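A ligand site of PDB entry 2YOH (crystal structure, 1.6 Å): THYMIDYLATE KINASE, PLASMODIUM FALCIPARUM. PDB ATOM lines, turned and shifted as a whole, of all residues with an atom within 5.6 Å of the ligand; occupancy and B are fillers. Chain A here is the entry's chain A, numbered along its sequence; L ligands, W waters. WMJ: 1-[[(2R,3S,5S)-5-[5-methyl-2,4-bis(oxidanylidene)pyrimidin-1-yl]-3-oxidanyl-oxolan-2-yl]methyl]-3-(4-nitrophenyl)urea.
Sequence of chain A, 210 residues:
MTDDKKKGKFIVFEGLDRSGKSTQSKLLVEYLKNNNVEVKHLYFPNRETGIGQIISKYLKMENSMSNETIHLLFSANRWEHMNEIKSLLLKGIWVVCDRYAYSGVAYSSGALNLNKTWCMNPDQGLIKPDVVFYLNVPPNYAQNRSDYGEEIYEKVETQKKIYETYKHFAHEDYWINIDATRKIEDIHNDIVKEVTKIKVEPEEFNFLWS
A nitrogen (NAO) of the ligand lies within hydrogen-bond range of the side-chain carboxylate (OE2) of Glu 151 (2.7 Å).
The guanidinium group (NH1) of Arg 78 is in hydrogen-bond range of an oxygen (OAC) of the ligand, at 2.8 Å.
N of Gly 104 lies close to OAC of the ligand, at 3.5 Å.
The guanidinium group of Arg 99 lies within hydrogen-bond range of an oxygen (OAB) of the ligand, at 2.7 Å.
NH2 of Arg 18 lies within hydrogen-bond range of OAF of the ligand (3.3 Å).
OH of Tyr 107 lies within hydrogen-bond range of OD1 of Asp 17, at 2.6 Å.
NH1 of Arg 78 sits at hydrogen-bond distance from O of Phe 74 (3.4 Å).
The side-chain hydroxyl of Tyr 107 lies within hydrogen-bond range of the guanidinium group of Arg 99, at 3.1 Å.
The side-chain hydroxyl of Ser 103 is in hydrogen-bond range of the guanidinium group of Arg 99 (2.9 Å).
The guanidinium group (NH2) of Arg 99 lies within salt-bridge range of the side-chain carboxylate (OD1) of Asp 17 (3.998 Å).
The backbone carbonyl oxygen of Gly 104 sits close to the side-chain hydroxyl of Ser 108 (3.3 Å).
Residues that only touch the ligand: Asp 17 (3.5 Å), Ser 22 (3.97 Å), Phe 44 (3.6 Å), Pro 45 (3.0 Å), Leu 59 (3.7 Å), Phe 74 (3.1 Å), Ser 103 (3.6 Å), Tyr 107 (3.1 Å) and Tyr 153 (3.8 Å).
14 residues have an atom within 4 Å of the ligand: Asp 17, Arg 18, Ser 22, Phe 44, Pro 45, Leu 59, Phe 74, Arg 78, Arg 99, Ser 103, Gly 104, Tyr 107, Glu 151 and Tyr 153.
Water W3 lies within hydrogen-bond range of a nitrogen (NAQ) of the ligand (2.8 Å), the side-chain hydroxyl (OG) of Ser 108 (3.1 Å) and the backbone carbonyl oxygen (O) of Gly 104 (3.2 Å).
Water W2 bridges the guanidinium group (NE) of Arg 99 and an oxygen (OAB) of the ligand.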
ATOM      1  N   LEU A  16      15.336  23.645   7.738  1.00  0.00           N
ATOM      2  CA  LEU A  16      15.910  23.153   6.514  1.00  0.00           C
ATOM      3  C   LEU A  16      17.210  22.418   6.787  1.00  0.00           C
ATOM      4  O   LEU A  16      17.744  22.495   7.848  1.00  0.00           O
ATOM      5  CB  LEU A  16      16.154  24.287   5.532  1.00  0.00           C
ATOM      6  CG  LEU A  16      14.900  24.890   4.844  1.00  0.00           C
ATOM      7  CD1 LEU A  16      15.364  26.026   3.907  1.00  0.00           C
ATOM      8  CD2 LEU A  16      14.153  23.866   4.037  1.00  0.00           C
ATOM      9  N   ASP A  17      17.738  21.759   5.745  1.00  0.00           N
ATOM     10  CA  ASP A  17      18.930  20.956   5.855  1.00  0.00           C
ATOM     11  C   ASP A  17      20.027  21.733   6.558  1.00  0.00           C
ATOM     12  O   ASP A  17      20.699  21.211   7.473  1.00  0.00           O
ATOM     13  CB  ASP A  17      19.432  20.492   4.451  1.00  0.00           C
ATOM     14  CG  ASP A  17      18.432  19.576   3.723  1.00  0.00           C
ATOM     15  OD1 ASP A  17      17.221  19.651   4.013  1.00  0.00           O
ATOM     16  OD2 ASP A  17      18.854  18.811   2.798  1.00  0.00           O
ATOM     17  N   ARG A  18      20.242  22.973   6.149  1.00  0.00           N
ATOM     18  CA  ARG A  18      21.395  23.661   6.718  1.00  0.00           C
ATOM     19  C   ARG A  18      21.064  24.678   7.827  1.00  0.00           C
ATOM     20  O   ARG A  18      21.580  25.795   7.851  1.00  0.00           O
ATOM     21  CB  ARG A  18      22.261  24.250   5.610  1.00  0.00           C
ATOM     22  CG  ARG A  18      23.082  23.143   4.856  1.00  0.00           C
ATOM     23  CD  ARG A  18      23.414  21.974   5.825  1.00  0.00           C
ATOM     24  NE  ARG A  18      24.691  21.286   5.597  1.00  0.00           N
ATOM     25  CZ  ARG A  18      24.891  20.305   4.714  1.00  0.00           C
ATOM     26  NH1 ARG A  18      23.905  19.886   3.925  1.00  0.00           N
ATOM     27  NH2 ARG A  18      26.084  19.738   4.619  1.00  0.00           N
ATOM     28  N   LYS A  21      20.224  22.376  13.382  1.00  0.00           N
ATOM     29  CA  LYS A  21      19.456  21.584  14.341  1.00  0.00           C
ATOM     30  C   LYS A  21      20.302  20.666  15.199  1.00  0.00           C
ATOM     31  O   LYS A  21      20.042  20.526  16.391  1.00  0.00           O
ATOM     32  CB  LYS A  21      18.355  20.760  13.651  1.00  0.00           C
ATOM     33  CG  LYS A  21      17.234  21.597  13.007  1.00  0.00           C
ATOM     34  CD  LYS A  21      16.234  20.691  12.301  1.00  0.00           C
ATOM     35  CE  LYS A  21      16.910  19.793  11.273  1.00  0.00           C
ATOM     36  NZ  LYS A  21      17.404  20.561  10.107  1.00  0.00           N
ATOM     37  N   SER A  22      21.322  20.028  14.622  1.00  0.00           N
ATOM     38  CA  SER A  22      22.087  19.094  15.446  1.00  0.00           C
ATOM     39  C   SER A  22      22.876  19.861  16.491  1.00  0.00           C
ATOM     40  O   SER A  22      22.993  19.392  17.613  1.00  0.00           O
ATOM     41  CB  SER A  22      22.970  18.131  14.647  1.00  0.00           C
ATOM     42  OG  SER A  22      23.922  18.839  13.876  1.00  0.00           O
ATOM     43  N   PHE A  44      15.020  11.871  13.620  1.00  0.00           N
ATOM     44  CA  PHE A  44      14.369  11.200  12.462  1.00  0.00           C
ATOM     45  C   PHE A  44      14.862  11.798  11.156  1.00  0.00           C
ATOM     46  O   PHE A  44      15.050  13.019  11.052  1.00  0.00           O
ATOM     47  CB  PHE A  44      12.807  11.379  12.527  1.00  0.00           C
ATOM     48  CG  PHE A  44      12.180  10.630  13.701  1.00  0.00           C
ATOM     49  CD1 PHE A  44      12.110   9.227  13.678  1.00  0.00           C
ATOM     50  CD2 PHE A  44      11.736  11.345  14.834  1.00  0.00           C
ATOM     51  CE1 PHE A  44      11.609   8.525  14.835  1.00  0.00           C
ATOM     52  CE2 PHE A  44      11.159  10.677  15.935  1.00  0.00           C
ATOM     53  CZ  PHE A  44      11.119   9.249  15.955  1.00  0.00           C
ATOM     54  N   PRO A  45      14.990  10.964  10.122  1.00  0.00           N
ATOM     55  CA  PRO A  45      14.844   9.508  10.191  1.00  0.00           C
ATOM     56  C   PRO A  45      15.993   8.897  10.982  1.00  0.00           C
ATOM     57  O   PRO A  45      17.030   9.605  11.263  1.00  0.00           O
ATOM     58  CB  PRO A  45      14.917   9.094   8.704  1.00  0.00           C
ATOM     59  CG  PRO A  45      15.886  10.147   8.060  1.00  0.00           C
ATOM     60  CD  PRO A  45      15.460  11.445   8.789  1.00  0.00           C
ATOM     61  N   ILE A  55      15.383   3.950   4.129  1.00  0.00           N
ATOM     62  CA  ILE A  55      15.396   5.403   4.024  1.00  0.00           C
ATOM     63  C   ILE A  55      16.808   5.913   3.695  1.00  0.00           C
ATOM     64  O   ILE A  55      16.961   6.768   2.871  1.00  0.00           O
ATOM     65  CB  ILE A  55      14.847   6.056   5.313  1.00  0.00           C
ATOM     66  CG1 ILE A  55      13.349   5.683   5.460  1.00  0.00           C
ATOM     67  CG2 ILE A  55      14.951   7.572   5.310  1.00  0.00           C
ATOM     68  CD1 ILE A  55      12.679   6.229   6.694  1.00  0.00           C
ATOM     69  N   LEU A  59      17.905   8.394   0.560  1.00  0.00           N
ATOM     70  CA  LEU A  59      18.521   9.687   0.714  1.00  0.00           C
ATOM     71  C   LEU A  59      19.782   9.819  -0.120  1.00  0.00           C
ATOM     72  O   LEU A  59      20.109  10.917  -0.638  1.00  0.00           O
ATOM     73  CB  LEU A  59      18.832   9.970   2.174  1.00  0.00           C
ATOM     74  CG  LEU A  59      17.541  10.241   2.966  1.00  0.00           C
ATOM     75  CD1 LEU A  59      17.874  10.312   4.449  1.00  0.00           C
ATOM     76  CD2 LEU A  59      16.806  11.541   2.476  1.00  0.00           C
ATOM     77  N   PHE A  74       8.910   7.031   6.035  1.00  0.00           N
ATOM     78  CA  PHE A  74       9.292   8.065   6.990  1.00  0.00           C
ATOM     79  C   PHE A  74       8.312   8.098   8.175  1.00  0.00           C
ATOM     80  O   PHE A  74       8.705   8.166   9.344  1.00  0.00           O
ATOM     81  CB  PHE A  74       9.313   9.451   6.322  1.00  0.00           C
ATOM     82  CG  PHE A  74      10.648   9.798   5.658  1.00  0.00           C
ATOM     83  CD1 PHE A  74      11.774  10.094   6.461  1.00  0.00           C
ATOM     84  CD2 PHE A  74      10.727   9.994   4.273  1.00  0.00           C
ATOM     85  CE1 PHE A  74      13.007  10.491   5.900  1.00  0.00           C
ATOM     86  CE2 PHE A  74      11.950  10.400   3.694  1.00  0.00           C
ATOM     87  CZ  PHE A  74      13.112  10.642   4.545  1.00  0.00           C
ATOM     88  N   SER A  75       7.014   7.952   7.887  1.00  0.00           N
ATOM     89  CA  SER A  75       6.009   7.925   8.984  1.00  0.00           C
ATOM     90  C   SER A  75       6.144   6.636   9.823  1.00  0.00           C
ATOM     91  O   SER A  75       6.111   6.717  11.025  1.00  0.00           O
ATOM     92  CB  SER A  75       4.570   8.121   8.413  1.00  0.00           C
ATOM     93  OG  SER A  75       3.644   7.995   9.452  1.00  0.00           O
ATOM     94  N   ARG A  78       8.676   6.862  12.580  1.00  0.00           N
ATOM     95  CA  ARG A  78       8.165   7.544  13.787  1.00  0.00           C
ATOM     96  C   ARG A  78       7.290   6.628  14.647  1.00  0.00           C
ATOM     97  O   ARG A  78       7.510   6.520  15.848  1.00  0.00           O
ATOM     98  CB  ARG A  78       7.429   8.823  13.406  1.00  0.00           C
ATOM     99  CG  ARG A  78       8.382   9.879  12.999  1.00  0.00           C
ATOM    100  CD  ARG A  78       7.637  11.154  12.588  1.00  0.00           C
ATOM    101  NE  ARG A  78       6.940  11.102  11.284  1.00  0.00           N
ATOM    102  CZ  ARG A  78       7.521  11.346  10.112  1.00  0.00           C
ATOM    103  NH1 ARG A  78       8.875  11.463   9.990  1.00  0.00           N
ATOM    104  NH2 ARG A  78       6.743  11.441   9.037  1.00  0.00           N
ATOM    105  N   ARG A  99      13.853  16.664  14.105  1.00  0.00           N
ATOM    106  CA  ARG A  99      12.858  16.359  13.050  1.00  0.00           C
ATOM    107  C   ARG A  99      11.745  15.457  13.533  1.00  0.00           C
ATOM    108  O   ARG A  99      11.948  14.598  14.365  1.00  0.00           O
ATOM    109  CB  ARG A  99      13.426  15.770  11.709  1.00  0.00           C
ATOM    110  CG  ARG A  99      14.509  16.645  11.073  1.00  0.00           C
ATOM    111  CD  ARG A  99      14.733  16.210   9.605  1.00  0.00           C
ATOM    112  NE  ARG A  99      15.733  17.068   8.975  1.00  0.00           N
ATOM    113  CZ  ARG A  99      15.451  18.251   8.442  1.00  0.00           C
ATOM    114  NH1 ARG A  99      14.186  18.725   8.500  1.00  0.00           N
ATOM    115  NH2 ARG A  99      16.433  18.971   7.873  1.00  0.00           N
ATOM    116  N   TYR A 100      10.568  15.688  12.987  1.00  0.00           N
ATOM    117  CA  TYR A 100       9.398  14.899  13.322  1.00  0.00           C
ATOM    118  C   TYR A 100       8.421  14.908  12.164  1.00  0.00           C
ATOM    119  O   TYR A 100       8.819  15.011  10.990  1.00  0.00           O
ATOM    120  CB  TYR A 100       8.763  15.457  14.564  1.00  0.00           C
ATOM    121  CG  TYR A 100       7.883  14.510  15.389  1.00  0.00           C
ATOM    122  CD1 TYR A 100       8.332  13.214  15.750  1.00  0.00           C
ATOM    123  CD2 TYR A 100       6.609  14.945  15.839  1.00  0.00           C
ATOM    124  CE1 TYR A 100       7.560  12.397  16.604  1.00  0.00           C
ATOM    125  CE2 TYR A 100       5.803  14.132  16.637  1.00  0.00           C
ATOM    126  CZ  TYR A 100       6.280  12.850  17.028  1.00  0.00           C
ATOM    127  OH  TYR A 100       5.499  12.076  17.880  1.00  0.00           O
ATOM    128  N   SER A 103       8.582  17.692   9.417  1.00  0.00           N
ATOM    129  CA  SER A 103       9.504  17.404   8.247  1.00  0.00           C
ATOM    130  C   SER A 103       8.833  16.528   7.231  1.00  0.00           C
ATOM    131  O   SER A 103       8.972  16.753   6.016  1.00  0.00           O
ATOM    132  CB  SER A 103      10.817  16.683   8.693  1.00  0.00           C
ATOM    133  OG  SER A 103      11.725  17.542   9.403  1.00  0.00           O
ATOM    134  N   GLY A 104       8.180  15.477   7.694  1.00  0.00           N
ATOM    135  CA  GLY A 104       7.415  14.557   6.825  1.00  0.00           C
ATOM    136  C   GLY A 104       6.554  15.329   5.802  1.00  0.00           C
ATOM    137  O   GLY A 104       6.587  15.065   4.600  1.00  0.00           O
ATOM    138  N   TYR A 107       8.691  18.313   3.606  1.00  0.00           N
ATOM    139  CA  TYR A 107       9.586  17.766   2.549  1.00  0.00           C
ATOM    140  C   TYR A 107       8.775  17.065   1.477  1.00  0.00           C
ATOM    141  O   TYR A 107       8.999  17.268   0.269  1.00  0.00           O
ATOM    142  CB  TYR A 107      10.637  16.834   3.165  1.00  0.00           C
ATOM    143  CG  TYR A 107      11.789  17.607   3.749  1.00  0.00           C
ATOM    144  CD1 TYR A 107      11.666  18.284   5.001  1.00  0.00           C
ATOM    145  CD2 TYR A 107      13.020  17.725   3.040  1.00  0.00           C
ATOM    146  CE1 TYR A 107      12.723  19.042   5.532  1.00  0.00           C
ATOM    147  CE2 TYR A 107      14.068  18.452   3.577  1.00  0.00           C
ATOM    148  CZ  TYR A 107      13.927  19.106   4.817  1.00  0.00           C
ATOM    149  OH  TYR A 107      14.982  19.893   5.312  1.00  0.00           O
ATOM    150  N   SER A 108       7.807  16.265   1.867  1.00  0.00           N
ATOM    151  CA  SER A 108       7.065  15.537   0.854  1.00  0.00           C
ATOM    152  C   SER A 108       6.169  16.463   0.024  1.00  0.00           C
ATOM    153  O   SER A 108       6.045  16.297  -1.184  1.00  0.00           O
ATOM    154  CB  SER A 108       6.218  14.426   1.453  1.00  0.00           C
ATOM    155  OG  SER A 108       7.104  13.386   1.836  1.00  0.00           O
ATOM    156  N   GLU A 151      23.089  14.553  -1.008  1.00  0.00           N
ATOM    157  CA  GLU A 151      21.728  14.112  -0.603  1.00  0.00           C
ATOM    158  C   GLU A 151      20.604  14.571  -1.534  1.00  0.00           C
ATOM    159  O   GLU A 151      20.683  15.631  -2.162  1.00  0.00           O
ATOM    160  CB  GLU A 151      21.432  14.565   0.816  1.00  0.00           C
ATOM    161  CG  GLU A 151      20.499  13.637   1.569  1.00  0.00           C
ATOM    162  CD  GLU A 151      20.314  14.048   3.008  1.00  0.00           C
ATOM    163  OE1 GLU A 151      21.227  13.770   3.822  1.00  0.00           O
ATOM    164  OE2 GLU A 151      19.249  14.626   3.355  1.00  0.00           O
ATOM    165  N   TYR A 153      17.649  16.077  -1.488  1.00  0.00           N
ATOM    166  CA  TYR A 153      16.920  17.386  -1.559  1.00  0.00           C
ATOM    167  C   TYR A 153      17.812  18.622  -1.428  1.00  0.00           C
ATOM    168  O   TYR A 153      17.314  19.733  -1.202  1.00  0.00           O
ATOM    169  CB  TYR A 153      15.885  17.440  -0.456  1.00  0.00           C
ATOM    170  CG  TYR A 153      14.861  16.352  -0.526  1.00  0.00           C
ATOM    171  CD1 TYR A 153      14.236  15.999  -1.756  1.00  0.00           C
ATOM    172  CD2 TYR A 153      14.486  15.672   0.630  1.00  0.00           C
ATOM    173  CE1 TYR A 153      13.281  14.980  -1.782  1.00  0.00           C
ATOM    174  CE2 TYR A 153      13.512  14.680   0.601  1.00  0.00           C
ATOM    175  CZ  TYR A 153      12.914  14.353  -0.587  1.00  0.00           C
ATOM    176  OH  TYR A 153      11.948  13.350  -0.548  1.00  0.00           O
HETATM  177  OAD WMJ L   1      11.720  14.038   3.904  1.00  0.00           O
HETATM  178  CAX WMJ L   1      11.779  13.823   5.096  1.00  0.00           C
HETATM  179  NAQ WMJ L   1      10.701  13.203   5.703  1.00  0.00           N
HETATM  180  CAW WMJ L   1      10.735  12.930   7.062  1.00  0.00           C
HETATM  181  OAC WMJ L   1       9.753  12.401   7.551  1.00  0.00           O
HETATM  182  CAT WMJ L   1      11.851  13.334   7.823  1.00  0.00           C
HETATM  183  CAA WMJ L   1      11.929  13.056   9.329  1.00  0.00           C
HETATM  184  CAL WMJ L   1      12.913  13.965   7.220  1.00  0.00           C
HETATM  185  NBC WMJ L   1      12.875  14.243   5.831  1.00  0.00           N
HETATM  186  CBA WMJ L   1      13.971  14.980   5.119  1.00  0.00           C
HETATM  187  OAR WMJ L   1      14.716  15.670   6.146  1.00  0.00           O
HETATM  188  CAN WMJ L   1      14.927  14.125   4.320  1.00  0.00           C
HETATM  189  CAY WMJ L   1      16.107  13.981   5.257  1.00  0.00           C
HETATM  190  OAE WMJ L   1      15.858  12.906   6.148  1.00  0.00           O
HETATM  191  CAZ WMJ L   1      16.103  15.286   6.038  1.00  0.00           C
HETATM  192  CAM WMJ L   1      16.786  16.452   5.264  1.00  0.00           C
HETATM  193  NAO WMJ L   1      18.234  16.203   5.232  1.00  0.00           N
HETATM  194  CAS WMJ L   1      19.072  16.854   6.088  1.00  0.00           C
HETATM  195  OAB WMJ L   1      18.675  17.682   6.939  1.00  0.00           O
HETATM  196  NAP WMJ L   1      20.366  16.605   5.871  1.00  0.00           N
HETATM  197  CAU WMJ L   1      21.417  17.132   6.579  1.00  0.00           C
HETATM  198  CAI WMJ L   1      22.694  16.945   6.057  1.00  0.00           C
HETATM  199  CAK WMJ L   1      23.818  17.462   6.734  1.00  0.00           C
HETATM  200  CAH WMJ L   1      21.252  17.819   7.776  1.00  0.00           C
HETATM  201  CAJ WMJ L   1      22.360  18.317   8.493  1.00  0.00           C
HETATM  202  CAV WMJ L   1      23.641  18.142   7.952  1.00  0.00           C
HETATM  203  NBB WMJ L   1      24.707  18.639   8.602  1.00  0.00           N
HETATM  204  OAG WMJ L   1      24.684  18.709   9.985  1.00  0.00           O
HETATM  205  OAF WMJ L   1      25.765  19.113   7.861  1.00  0.00           O
HETATM  206  O   HOH W   1      18.381  12.760   7.158  1.00  0.00           O
HETATM  207  O   HOH W   2      18.223  15.220   9.142  1.00  0.00           O
HETATM  208  O   HOH W   3       8.349  12.431   4.456  1.00  0.00           O
